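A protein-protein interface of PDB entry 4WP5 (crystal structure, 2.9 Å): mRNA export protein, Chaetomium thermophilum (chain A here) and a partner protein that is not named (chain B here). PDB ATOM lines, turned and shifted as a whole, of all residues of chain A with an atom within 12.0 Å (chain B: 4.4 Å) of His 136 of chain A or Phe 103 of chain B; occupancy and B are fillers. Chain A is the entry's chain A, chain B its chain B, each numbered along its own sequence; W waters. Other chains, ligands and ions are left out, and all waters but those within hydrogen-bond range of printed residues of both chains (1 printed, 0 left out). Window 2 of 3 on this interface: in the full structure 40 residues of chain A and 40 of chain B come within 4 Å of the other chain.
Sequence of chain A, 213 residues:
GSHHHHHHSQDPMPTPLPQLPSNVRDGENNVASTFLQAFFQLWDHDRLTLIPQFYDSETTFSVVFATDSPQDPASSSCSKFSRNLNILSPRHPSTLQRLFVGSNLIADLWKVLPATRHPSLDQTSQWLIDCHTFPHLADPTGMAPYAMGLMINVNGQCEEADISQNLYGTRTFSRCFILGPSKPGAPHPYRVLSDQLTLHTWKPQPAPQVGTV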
ATOM      1  N   HIS A 132     -33.308  26.265 -27.521  1.00  0.00           N
ATOM      2  CA  HIS A 132     -32.237  27.242 -27.352  1.00  0.00           C
ATOM      3  C   HIS A 132     -31.038  26.614 -26.650  1.00  0.00           C
ATOM      4  O   HIS A 132     -31.117  25.493 -26.144  1.00  0.00           O
ATOM      5  CB  HIS A 132     -32.729  28.462 -26.563  1.00  0.00           C
ATOM      6  CG  HIS A 132     -32.848  28.229 -25.087  1.00  0.00           C
ATOM      7  ND1 HIS A 132     -34.063  28.090 -24.455  1.00  0.00           N
ATOM      8  CD2 HIS A 132     -31.905  28.125 -24.121  1.00  0.00           C
ATOM      9  CE1 HIS A 132     -33.865  27.896 -23.162  1.00  0.00           C
ATOM     10  NE2 HIS A 132     -32.566  27.914 -22.934  1.00  0.00           N
ATOM     11  N   THR A 133     -29.933  27.353 -26.620  1.00  0.00           N
ATOM     12  CA  THR A 133     -28.708  26.907 -25.967  1.00  0.00           C
ATOM     13  C   THR A 133     -28.526  27.597 -24.619  1.00  0.00           C
ATOM     14  O   THR A 133     -28.757  28.800 -24.496  1.00  0.00           O
ATOM     15  CB  THR A 133     -27.471  27.187 -26.838  1.00  0.00           C
ATOM     16  OG1 THR A 133     -27.393  28.591 -27.119  1.00  0.00           O
ATOM     17  CG2 THR A 133     -27.543  26.412 -28.147  1.00  0.00           C
ATOM     18  N   PHE A 134     -28.103  26.829 -23.617  1.00  0.00           N
ATOM     19  CA  PHE A 134     -27.921  27.344 -22.263  1.00  0.00           C
ATOM     20  C   PHE A 134     -26.554  26.934 -21.715  1.00  0.00           C
ATOM     21  O   PHE A 134     -25.964  25.963 -22.188  1.00  0.00           O
ATOM     22  CB  PHE A 134     -29.035  26.838 -21.346  1.00  0.00           C
ATOM     23  CG  PHE A 134     -29.101  25.342 -21.246  1.00  0.00           C
ATOM     24  CD1 PHE A 134     -28.496  24.679 -20.193  1.00  0.00           C
ATOM     25  CD2 PHE A 134     -29.762  24.597 -22.210  1.00  0.00           C
ATOM     26  CE1 PHE A 134     -28.551  23.305 -20.099  1.00  0.00           C
ATOM     27  CE2 PHE A 134     -29.819  23.219 -22.120  1.00  0.00           C
ATOM     28  CZ  PHE A 134     -29.212  22.574 -21.064  1.00  0.00           C
ATOM     29  N   PRO A 135     -26.046  27.673 -20.713  1.00  0.00           N
ATOM     30  CA  PRO A 135     -24.687  27.457 -20.208  1.00  0.00           C
ATOM     31  C   PRO A 135     -24.596  26.544 -18.984  1.00  0.00           C
ATOM     32  O   PRO A 135     -25.606  26.030 -18.505  1.00  0.00           O
ATOM     33  CB  PRO A 135     -24.251  28.869 -19.834  1.00  0.00           C
ATOM     34  CG  PRO A 135     -25.516  29.491 -19.316  1.00  0.00           C
ATOM     35  CD  PRO A 135     -26.655  28.872 -20.107  1.00  0.00           C
ATOM     36  N   HIS A 136     -23.368  26.350 -18.507  1.00  0.00           N
ATOM     37  CA  HIS A 136     -23.103  25.750 -17.201  1.00  0.00           C
ATOM     38  C   HIS A 136     -23.471  24.270 -17.111  1.00  0.00           C
ATOM     39  O   HIS A 136     -23.698  23.750 -16.020  1.00  0.00           O
ATOM     40  CB  HIS A 136     -23.840  26.540 -16.118  1.00  0.00           C
ATOM     41  CG  HIS A 136     -23.565  28.009 -16.167  1.00  0.00           C
ATOM     42  ND1 HIS A 136     -24.488  28.957 -15.775  1.00  0.00           N
ATOM     43  CD2 HIS A 136     -22.470  28.696 -16.566  1.00  0.00           C
ATOM     44  CE1 HIS A 136     -23.971  30.161 -15.932  1.00  0.00           C
ATOM     45  NE2 HIS A 136     -22.745  30.031 -16.411  1.00  0.00           N
ATOM     46  N   LEU A 137     -23.512  23.594 -18.254  1.00  0.00           N
ATOM     47  CA  LEU A 137     -23.658  22.144 -18.275  1.00  0.00           C
ATOM     48  C   LEU A 137     -22.332  21.523 -17.852  1.00  0.00           C
ATOM     49  O   LEU A 137     -21.333  22.229 -17.724  1.00  0.00           O
ATOM     50  CB  LEU A 137     -24.066  21.657 -19.666  1.00  0.00           C
ATOM     51  CG  LEU A 137     -24.945  20.407 -19.744  1.00  0.00           C
ATOM     52  CD1 LEU A 137     -26.283  20.657 -19.071  1.00  0.00           C
ATOM     53  CD2 LEU A 137     -25.139  19.996 -21.194  1.00  0.00           C
ATOM     54  N   ALA A 138     -22.314  20.212 -17.634  1.00  0.00           N
ATOM     55  CA  ALA A 138     -21.080  19.532 -17.252  1.00  0.00           C
ATOM     56  C   ALA A 138     -20.260  19.197 -18.493  1.00  0.00           C
ATOM     57  O   ALA A 138     -20.818  18.956 -19.563  1.00  0.00           O
ATOM     58  CB  ALA A 138     -21.383  18.273 -16.457  1.00  0.00           C
ATOM     59  N   ASP A 139     -18.939  19.191 -18.340  1.00  0.00           N
ATOM     60  CA  ASP A 139     -18.025  18.911 -19.445  1.00  0.00           C
ATOM     61  C   ASP A 139     -17.489  17.478 -19.357  1.00  0.00           C
ATOM     62  O   ASP A 139     -16.665  17.183 -18.492  1.00  0.00           O
ATOM     63  CB  ASP A 139     -16.869  19.911 -19.438  1.00  0.00           C
ATOM     64  CG  ASP A 139     -15.919  19.718 -20.605  1.00  0.00           C
ATOM     65  OD1 ASP A 139     -16.346  19.162 -21.638  1.00  0.00           O
ATOM     66  OD2 ASP A 139     -14.744  20.126 -20.493  1.00  0.00           O
ATOM     67  N   PRO A 140     -17.954  16.583 -20.250  1.00  0.00           N
ATOM     68  CA  PRO A 140     -17.523  15.180 -20.178  1.00  0.00           C
ATOM     69  C   PRO A 140     -16.025  14.988 -20.410  1.00  0.00           C
ATOM     70  O   PRO A 140     -15.444  14.042 -19.878  1.00  0.00           O
ATOM     71  CB  PRO A 140     -18.328  14.504 -21.297  1.00  0.00           C
ATOM     72  CG  PRO A 140     -19.455  15.422 -21.585  1.00  0.00           C
ATOM     73  CD  PRO A 140     -18.942  16.794 -21.321  1.00  0.00           C
ATOM     74  N   ALA A 144     -12.538  21.368 -18.879  1.00  0.00           N
ATOM     75  CA  ALA A 144     -13.139  22.642 -18.495  1.00  0.00           C
ATOM     76  C   ALA A 144     -14.226  22.418 -17.450  1.00  0.00           C
ATOM     77  O   ALA A 144     -14.819  21.342 -17.393  1.00  0.00           O
ATOM     78  CB  ALA A 144     -13.709  23.348 -19.719  1.00  0.00           C
ATOM     79  N   PRO A 145     -14.491  23.433 -16.612  1.00  0.00           N
ATOM     80  CA  PRO A 145     -15.545  23.298 -15.600  1.00  0.00           C
ATOM     81  C   PRO A 145     -16.930  23.158 -16.215  1.00  0.00           C
ATOM     82  O   PRO A 145     -17.675  22.248 -15.847  1.00  0.00           O
ATOM     83  CB  PRO A 145     -15.437  24.599 -14.799  1.00  0.00           C
ATOM     84  CG  PRO A 145     -14.778  25.563 -15.720  1.00  0.00           C
ATOM     85  CD  PRO A 145     -13.837  24.752 -16.553  1.00  0.00           C
ATOM     86  N   TYR A 146     -17.259  24.048 -17.146  1.00  0.00           N
ATOM     87  CA  TYR A 146     -18.586  24.073 -17.748  1.00  0.00           C
ATOM     88  C   TYR A 146     -18.572  23.723 -19.229  1.00  0.00           C
ATOM     89  O   TYR A 146     -17.531  23.748 -19.885  1.00  0.00           O
ATOM     90  CB  TYR A 146     -19.220  25.452 -17.569  1.00  0.00           C
ATOM     91  CG  TYR A 146     -19.105  25.996 -16.168  1.00  0.00           C
ATOM     92  CD1 TYR A 146     -19.957  25.561 -15.162  1.00  0.00           C
ATOM     93  CD2 TYR A 146     -18.147  26.948 -15.851  1.00  0.00           C
ATOM     94  CE1 TYR A 146     -19.854  26.058 -13.878  1.00  0.00           C
ATOM     95  CE2 TYR A 146     -18.037  27.450 -14.571  1.00  0.00           C
ATOM     96  CZ  TYR A 146     -18.892  27.003 -13.588  1.00  0.00           C
ATOM     97  OH  TYR A 146     -18.781  27.505 -12.313  1.00  0.00           O
ATOM     98  N   ALA A 147     -19.755  23.398 -19.736  1.00  0.00           N
ATOM     99  CA  ALA A 147     -19.974  23.186 -21.158  1.00  0.00           C
ATOM    100  C   ALA A 147     -21.368  23.704 -21.489  1.00  0.00           C
ATOM    101  O   ALA A 147     -22.201  23.855 -20.597  1.00  0.00           O
ATOM    102  CB  ALA A 147     -19.830  21.719 -21.521  1.00  0.00           C
ATOM    103  N   MET A 148     -21.616  23.982 -22.765  1.00  0.00           N
ATOM    104  CA  MET A 148     -22.891  24.553 -23.185  1.00  0.00           C
ATOM    105  C   MET A 148     -23.813  23.466 -23.725  1.00  0.00           C
ATOM    106  O   MET A 148     -23.368  22.555 -24.423  1.00  0.00           O
ATOM    107  CB  MET A 148     -22.662  25.636 -24.237  1.00  0.00           C
ATOM    108  CG  MET A 148     -23.671  26.769 -24.184  1.00  0.00           C
ATOM    109  SD  MET A 148     -23.063  28.274 -24.961  1.00  0.00           S
ATOM    110  CE  MET A 148     -24.306  29.449 -24.431  1.00  0.00           C
ATOM    111  N   GLY A 149     -25.096  23.569 -23.391  1.00  0.00           N
ATOM    112  CA  GLY A 149     -26.080  22.573 -23.779  1.00  0.00           C
ATOM    113  C   GLY A 149     -27.163  23.147 -24.670  1.00  0.00           C
ATOM    114  O   GLY A 149     -27.244  24.360 -24.854  1.00  0.00           O
ATOM    115  N   LEU A 150     -27.993  22.265 -25.221  1.00  0.00           N
ATOM    116  CA  LEU A 150     -29.083  22.652 -26.112  1.00  0.00           C
ATOM    117  C   LEU A 150     -30.400  22.036 -25.648  1.00  0.00           C
ATOM    118  O   LEU A 150     -30.562  20.816 -25.676  1.00  0.00           O
ATOM    119  CB  LEU A 150     -28.776  22.214 -27.550  1.00  0.00           C
ATOM    120  CG  LEU A 150     -29.848  22.445 -28.620  1.00  0.00           C
ATOM    121  CD1 LEU A 150     -29.991  23.924 -28.946  1.00  0.00           C
ATOM    122  CD2 LEU A 150     -29.528  21.643 -29.874  1.00  0.00           C
ATOM    123  N   MET A 151     -31.335  22.879 -25.219  1.00  0.00           N
ATOM    124  CA  MET A 151     -32.660  22.417 -24.812  1.00  0.00           C
ATOM    125  C   MET A 151     -33.606  22.461 -26.004  1.00  0.00           C
ATOM    126  O   MET A 151     -33.671  23.470 -26.702  1.00  0.00           O
ATOM    127  CB  MET A 151     -33.210  23.277 -23.672  1.00  0.00           C
ATOM    128  CG  MET A 151     -34.639  22.931 -23.267  1.00  0.00           C
ATOM    129  SD  MET A 151     -35.264  23.949 -21.916  1.00  0.00           S
ATOM    130  CE  MET A 151     -35.181  22.794 -20.552  1.00  0.00           C
ATOM    131  N   ILE A 178     -32.769  17.346 -23.595  1.00  0.00           N
ATOM    132  CA  ILE A 178     -31.595  18.096 -23.159  1.00  0.00           C
ATOM    133  C   ILE A 178     -30.356  17.514 -23.824  1.00  0.00           C
ATOM    134  O   ILE A 178     -29.890  16.435 -23.456  1.00  0.00           O
ATOM    135  CB  ILE A 178     -31.416  18.073 -21.632  1.00  0.00           C
ATOM    136  CG1 ILE A 178     -32.613  18.731 -20.939  1.00  0.00           C
ATOM    137  CG2 ILE A 178     -30.129  18.790 -21.252  1.00  0.00           C
ATOM    138  CD1 ILE A 178     -32.754  20.221 -21.210  1.00  0.00           C
ATOM    139  N   LEU A 179     -29.838  18.233 -24.815  1.00  0.00           N
ATOM    140  CA  LEU A 179     -28.659  17.803 -25.555  1.00  0.00           C
ATOM    141  C   LEU A 179     -27.403  18.466 -25.002  1.00  0.00           C
ATOM    142  O   LEU A 179     -27.438  19.614 -24.562  1.00  0.00           O
ATOM    143  CB  LEU A 179     -28.816  18.128 -27.042  1.00  0.00           C
ATOM    144  CG  LEU A 179     -29.316  16.996 -27.943  1.00  0.00           C
ATOM    145  CD1 LEU A 179     -30.552  16.322 -27.368  1.00  0.00           C
ATOM    146  CD2 LEU A 179     -29.607  17.540 -29.332  1.00  0.00           C
ATOM    147  N   GLY A 180     -26.297  17.729 -25.018  1.00  0.00           N
ATOM    148  CA  GLY A 180     -25.028  18.246 -24.545  1.00  0.00           C
ATOM    149  C   GLY A 180     -23.868  17.580 -25.255  1.00  0.00           C
ATOM    150  O   GLY A 180     -24.071  16.651 -26.037  1.00  0.00           O
ATOM    151  N   PRO A 181     -22.640  18.052 -24.990  1.00  0.00           N
ATOM    152  CA  PRO A 181     -21.450  17.429 -25.579  1.00  0.00           C
ATOM    153  C   PRO A 181     -21.298  15.986 -25.111  1.00  0.00           C
ATOM    154  O   PRO A 181     -21.651  15.674 -23.974  1.00  0.00           O
ATOM    155  CB  PRO A 181     -20.301  18.312 -25.077  1.00  0.00           C
ATOM    156  CG  PRO A 181     -20.830  18.983 -23.858  1.00  0.00           C
ATOM    157  CD  PRO A 181     -22.298  19.162 -24.084  1.00  0.00           C
ATOM    158  N   ARG A 191     -24.833  14.338 -27.234  1.00  0.00           N
ATOM    159  CA  ARG A 191     -25.580  13.247 -26.626  1.00  0.00           C
ATOM    160  C   ARG A 191     -26.849  13.774 -25.972  1.00  0.00           C
ATOM    161  O   ARG A 191     -26.966  14.970 -25.710  1.00  0.00           O
ATOM    162  CB  ARG A 191     -24.725  12.529 -25.584  1.00  0.00           C
ATOM    163  CG  ARG A 191     -24.370  13.407 -24.390  1.00  0.00           C
ATOM    164  CD  ARG A 191     -23.594  12.652 -23.326  1.00  0.00           C
ATOM    165  NE  ARG A 191     -23.380  13.478 -22.141  1.00  0.00           N
ATOM    166  CZ  ARG A 191     -22.661  13.109 -21.085  1.00  0.00           C
ATOM    167  NH1 ARG A 191     -22.073  11.922 -21.057  1.00  0.00           N
ATOM    168  NH2 ARG A 191     -22.529  13.933 -20.055  1.00  0.00           N
ATOM    169  N   LEU A 193     -28.880  14.137 -22.699  1.00  0.00           N
ATOM    170  CA  LEU A 193     -28.701  14.087 -21.250  1.00  0.00           C
ATOM    171  C   LEU A 193     -29.996  13.690 -20.554  1.00  0.00           C
ATOM    172  O   LEU A 193     -29.978  12.941 -19.579  1.00  0.00           O
ATOM    173  CB  LEU A 193     -28.221  15.437 -20.712  1.00  0.00           C
ATOM    174  CG  LEU A 193     -26.730  15.548 -20.383  1.00  0.00           C
ATOM    175  CD1 LEU A 193     -25.893  15.598 -21.650  1.00  0.00           C
ATOM    176  CD2 LEU A 193     -26.472  16.766 -19.510  1.00  0.00           C
ATOM    177  N   TYR B  36     -25.921  35.654  -8.500  1.00  0.00           N
ATOM    178  CA  TYR B  36     -25.747  35.246  -9.889  1.00  0.00           C
ATOM    179  C   TYR B  36     -25.391  36.433 -10.778  1.00  0.00           C
ATOM    180  O   TYR B  36     -24.557  36.316 -11.675  1.00  0.00           O
ATOM    181  CB  TYR B  36     -27.015  34.566 -10.409  1.00  0.00           C
ATOM    182  CG  TYR B  36     -27.088  33.090 -10.088  1.00  0.00           C
ATOM    183  CD1 TYR B  36     -26.554  32.147 -10.956  1.00  0.00           C
ATOM    184  CD2 TYR B  36     -27.690  32.640  -8.922  1.00  0.00           C
ATOM    185  CE1 TYR B  36     -26.617  30.798 -10.672  1.00  0.00           C
ATOM    186  CE2 TYR B  36     -27.758  31.290  -8.628  1.00  0.00           C
ATOM    187  CZ  TYR B  36     -27.220  30.374  -9.507  1.00  0.00           C
ATOM    188  OH  TYR B  36     -27.283  29.030  -9.221  1.00  0.00           O
ATOM    189  N   ALA B  39     -21.946  37.207 -10.107  1.00  0.00           N
ATOM    190  CA  ALA B  39     -21.108  36.158 -10.676  1.00  0.00           C
ATOM    191  C   ALA B  39     -21.021  36.286 -12.194  1.00  0.00           C
ATOM    192  O   ALA B  39     -20.140  35.701 -12.827  1.00  0.00           O
ATOM    193  CB  ALA B  39     -21.645  34.788 -10.292  1.00  0.00           C
ATOM    194  N   GLY B  40     -21.939  37.054 -12.772  1.00  0.00           N
ATOM    195  CA  GLY B  40     -21.962  37.268 -14.205  1.00  0.00           C
ATOM    196  C   GLY B  40     -22.761  36.196 -14.918  1.00  0.00           C
ATOM    197  O   GLY B  40     -22.249  35.520 -15.810  1.00  0.00           O
ATOM    198  N   HIS B  41     -24.018  36.036 -14.515  1.00  0.00           N
ATOM    199  CA  HIS B  41     -24.918  35.084 -15.156  1.00  0.00           C
ATOM    200  C   HIS B  41     -25.755  35.791 -16.221  1.00  0.00           C
ATOM    201  O   HIS B  41     -26.220  36.908 -15.994  1.00  0.00           O
ATOM    202  CB  HIS B  41     -25.833  34.423 -14.122  1.00  0.00           C
ATOM    203  CG  HIS B  41     -26.622  33.273 -14.663  1.00  0.00           C
ATOM    204  ND1 HIS B  41     -27.784  33.440 -15.389  1.00  0.00           N
ATOM    205  CD2 HIS B  41     -26.420  31.937 -14.586  1.00  0.00           C
ATOM    206  CE1 HIS B  41     -28.259  32.259 -15.735  1.00  0.00           C
ATOM    207  NE2 HIS B  41     -27.449  31.328 -15.260  1.00  0.00           N
ATOM    208  N   ASN B  98     -27.192  18.413 -14.308  1.00  0.00           N
ATOM    209  CA  ASN B  98     -25.865  18.600 -13.732  1.00  0.00           C
ATOM    210  C   ASN B  98     -25.874  18.169 -12.276  1.00  0.00           C
ATOM    211  O   ASN B  98     -26.592  18.737 -11.458  1.00  0.00           O
ATOM    212  CB  ASN B  98     -25.404  20.054 -13.843  1.00  0.00           C
ATOM    213  CG  ASN B  98     -23.903  20.202 -13.658  1.00  0.00           C
ATOM    214  OD1 ASN B  98     -23.237  19.294 -13.160  1.00  0.00           O
ATOM    215  ND2 ASN B  98     -23.364  21.349 -14.059  1.00  0.00           N
ATOM    216  N   TYR B 101     -23.122  21.199  -9.991  1.00  0.00           N
ATOM    217  CA  TYR B 101     -23.296  22.603 -10.365  1.00  0.00           C
ATOM    218  C   TYR B 101     -22.560  23.503  -9.374  1.00  0.00           C
ATOM    219  O   TYR B 101     -22.860  23.488  -8.181  1.00  0.00           O
ATOM    220  CB  TYR B 101     -24.788  22.960 -10.413  1.00  0.00           C
ATOM    221  CG  TYR B 101     -25.099  24.283 -11.073  1.00  0.00           C
ATOM    222  CD1 TYR B 101     -25.033  24.429 -12.452  1.00  0.00           C
ATOM    223  CD2 TYR B 101     -25.480  25.383 -10.319  1.00  0.00           C
ATOM    224  CE1 TYR B 101     -25.324  25.636 -13.059  1.00  0.00           C
ATOM    225  CE2 TYR B 101     -25.775  26.593 -10.916  1.00  0.00           C
ATOM    226  CZ  TYR B 101     -25.696  26.713 -12.286  1.00  0.00           C
ATOM    227  OH  TYR B 101     -25.987  27.917 -12.885  1.00  0.00           O
ATOM    228  N   ARG B 102     -21.604  24.284  -9.875  1.00  0.00           N
ATOM    229  CA  ARG B 102     -20.739  25.099  -9.023  1.00  0.00           C
ATOM    230  C   ARG B 102     -20.808  26.591  -9.335  1.00  0.00           C
ATOM    231  O   ARG B 102     -20.153  27.393  -8.669  1.00  0.00           O
ATOM    232  CB  ARG B 102     -19.285  24.635  -9.154  1.00  0.00           C
ATOM    233  CG  ARG B 102     -19.037  23.203  -8.713  1.00  0.00           C
ATOM    234  CD  ARG B 102     -17.547  22.919  -8.595  1.00  0.00           C
ATOM    235  NE  ARG B 102     -17.277  21.570  -8.106  1.00  0.00           N
ATOM    236  CZ  ARG B 102     -16.059  21.089  -7.872  1.00  0.00           C
ATOM    237  NH1 ARG B 102     -14.989  21.843  -8.081  1.00  0.00           N
ATOM    238  NH2 ARG B 102     -15.911  19.848  -7.426  1.00  0.00           N
ATOM    239  N   PHE B 103     -21.590  26.969 -10.338  1.00  0.00           N
ATOM    240  CA  PHE B 103     -21.596  28.356 -10.792  1.00  0.00           C
ATOM    241  C   PHE B 103     -22.172  29.302  -9.739  1.00  0.00           C
ATOM    242  O   PHE B 103     -23.225  29.037  -9.159  1.00  0.00           O
ATOM    243  CB  PHE B 103     -22.382  28.495 -12.097  1.00  0.00           C
ATOM    244  CG  PHE B 103     -22.326  29.875 -12.684  1.00  0.00           C
ATOM    245  CD1 PHE B 103     -21.284  30.244 -13.519  1.00  0.00           C
ATOM    246  CD2 PHE B 103     -23.306  30.806 -12.390  1.00  0.00           C
ATOM    247  CE1 PHE B 103     -21.226  31.518 -14.054  1.00  0.00           C
ATOM    248  CE2 PHE B 103     -23.253  32.079 -12.921  1.00  0.00           C
ATOM    249  CZ  PHE B 103     -22.212  32.435 -13.755  1.00  0.00           C
ATOM    250  N   ALA B 104     -21.458  30.400  -9.504  1.00  0.00           N
ATOM    251  CA  ALA B 104     -21.870  31.445  -8.565  1.00  0.00           C
ATOM    252  C   ALA B 104     -21.926  30.933  -7.130  1.00  0.00           C
ATOM    253  O   ALA B 104     -22.546  31.559  -6.269  1.00  0.00           O
ATOM    254  CB  ALA B 104     -23.223  32.022  -8.971  1.00  0.00           C
ATOM    255  N   ALA B 105     -21.267  29.807  -6.873  1.00  0.00           N
ATOM    256  CA  ALA B 105     -21.304  29.179  -5.556  1.00  0.00           C
ATOM    257  C   ALA B 105     -20.099  29.577  -4.703  1.00  0.00           C
ATOM    258  O   ALA B 105     -18.980  29.657  -5.211  1.00  0.00           O
ATOM    259  CB  ALA B 105     -21.356  27.672  -5.699  1.00  0.00           C
ATOM    260  N   MET B 122     -28.439  21.102 -11.118  1.00  0.00           N
ATOM    261  CA  MET B 122     -29.168  21.829 -12.149  1.00  0.00           C
ATOM    262  C   MET B 122     -30.253  20.913 -12.696  1.00  0.00           C
ATOM    263  O   MET B 122     -29.960  19.807 -13.152  1.00  0.00           O
ATOM    264  CB  MET B 122     -28.230  22.275 -13.273  1.00  0.00           C
ATOM    265  CG  MET B 122     -28.664  23.552 -13.973  1.00  0.00           C
ATOM    266  SD  MET B 122     -28.312  23.566 -15.742  1.00  0.00           S
ATOM    267  CE  MET B 122     -26.584  23.109 -15.744  1.00  0.00           C
ATOM    268  N   TRP B 159     -27.802  29.837  -3.897  1.00  0.00           N
ATOM    269  CA  TRP B 159     -26.738  29.674  -2.908  1.00  0.00           C
ATOM    270  C   TRP B 159     -26.978  30.468  -1.627  1.00  0.00           C
ATOM    271  O   TRP B 159     -26.521  30.079  -0.553  1.00  0.00           O
ATOM    272  CB  TRP B 159     -25.401  30.080  -3.528  1.00  0.00           C
ATOM    273  CG  TRP B 159     -25.191  29.457  -4.868  1.00  0.00           C
ATOM    274  CD1 TRP B 159     -25.237  30.079  -6.082  1.00  0.00           C
ATOM    275  CD2 TRP B 159     -24.932  28.081  -5.132  1.00  0.00           C
ATOM    276  NE1 TRP B 159     -25.010  29.171  -7.088  1.00  0.00           N
ATOM    277  CE2 TRP B 159     -24.819  27.932  -6.527  1.00  0.00           C
ATOM    278  CE3 TRP B 159     -24.778  26.953  -4.321  1.00  0.00           C
ATOM    279  CZ2 TRP B 159     -24.558  26.706  -7.131  1.00  0.00           C
ATOM    280  CZ3 TRP B 159     -24.519  25.743  -4.916  1.00  0.00           C
ATOM    281  CH2 TRP B 159     -24.411  25.624  -6.307  1.00  0.00           C
HETATM  282  O   HOH W   1     -27.150  28.731 -15.661  1.00  0.00           O
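Of the 23 printed residues of chain A, 4 touch a printed residue of chain B. Printed residues of chain A that touch a printed residue of chain B: His 136, Leu 137, Ala 138 and Tyr 146. Along chain B the printed residues that touch a printed residue of chain A span positions 41 to 122. Among the printed residues, 10 pairs touch across the chains. Among the printed residues, no Asp or Glu carboxylate lies within 4 Å of a Lys or Arg side-chain nitrogen of the other chain.
Phe 103 of chain B touches just these residues of chain A: His 136 (3.2 Å) and Tyr 146 (3.3 Å). No residue of chain A comes within 4 Å of Tyr 36 of chain B. No residue of chain A comes within 4 Å of Ala 39 of chain B. No residue of chain A comes within 4 Å of Gly 40 of chain B. Of chain A, only His 136 (3.3 Å) comes within 4 Å of His 41 of chain B. Of chain A, only His 136 comes within 4 Å of Tyr 101 of chain B. No residue of chain A comes within 4 Å of Ala 104 of chain B. No residue of chain A comes within 4 Å of Ala 105 of chain B. Of the printed residues of chain B, Tyr 146 of chain A touches Arg 102 (3.7 Å) and Phe 103 (3.3 Å). Printed residues of chain B within 4 Å of Ala 138 of chain A: Asn 98 (3.9 Å). Of the printed residues of chain B, Leu 137 of chain A touches Asn 98 (3.9 Å) and Met 122 (3.99 Å). Phe 134 of chain A touches none of the printed residues of chain B. The nearest residue of chain A that does not touch Phe 103 of chain B is Pro 135 of chain A (7.0 Å). The nearest printed residue of chain B that does not touch Ala 138 of chain A is Met 122 of chain B (5.5 Å).
The backbone carbonyl oxygen of Ala 147 of chain A sits at hydrogen-bond distance from the backbone NH of His 136 of chain A, 3.5 Å away. The backbone NH (N) of Leu 137 of chain A sits at hydrogen-bond distance from the backbone carbonyl oxygen (O) of Ala 147 of chain A, 2.7 Å away. O of Tyr 36 of chain B lies within hydrogen-bond range of N of His 41 of chain B. N of Met 122 of chain B sits at hydrogen-bond distance from O of Asn 98 of chain B (3.0 Å). The backbone carbonyl oxygen (O) of Phe 103 of chain B lies within hydrogen-bond range of the indole nitrogen (NE1) of Trp 159 of chain B (2.7 Å).
The backbone carbonyl oxygen of His 136 of chain A is in hydrogen-bond range of the side-chain amide nitrogen of Asn 98 of chain B, at 3.1 Å. A ring nitrogen (ND1) of His 136 of chain A lies within hydrogen-bond range of the side-chain hydroxyl of Tyr 101 of chain B (3.4 Å). OH of Tyr 146 of chain A lies close to N of Phe 103 of chain B (3.5 Å).
His 136 of chain A touches His 41 of chain B. His 136 of chain A touches Phe 103 of chain B (NE2 to CE1, 3.2 Å). Met 122 of chain B touches His 136 of chain A (CE to O, 3.0 Å). Asn 98 of chain B touches Leu 137 of chain A (ND2 to C, 3.9 Å). Leu 137 of chain A touches Met 122 of chain B. Ala 138 of chain A touches Asn 98 of chain B (N to ND2, 3.9 Å). OH of Tyr 146 of chain A touches C of Arg 102 of chain B, at 3.7 Å.
Water W1 lies within hydrogen-bond range of NE2 of His 41 of chain B (2.6 Å), ND1 of His 136 of chain A (2.7 Å) and OH of Tyr 101 of chain B (3.1 Å).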
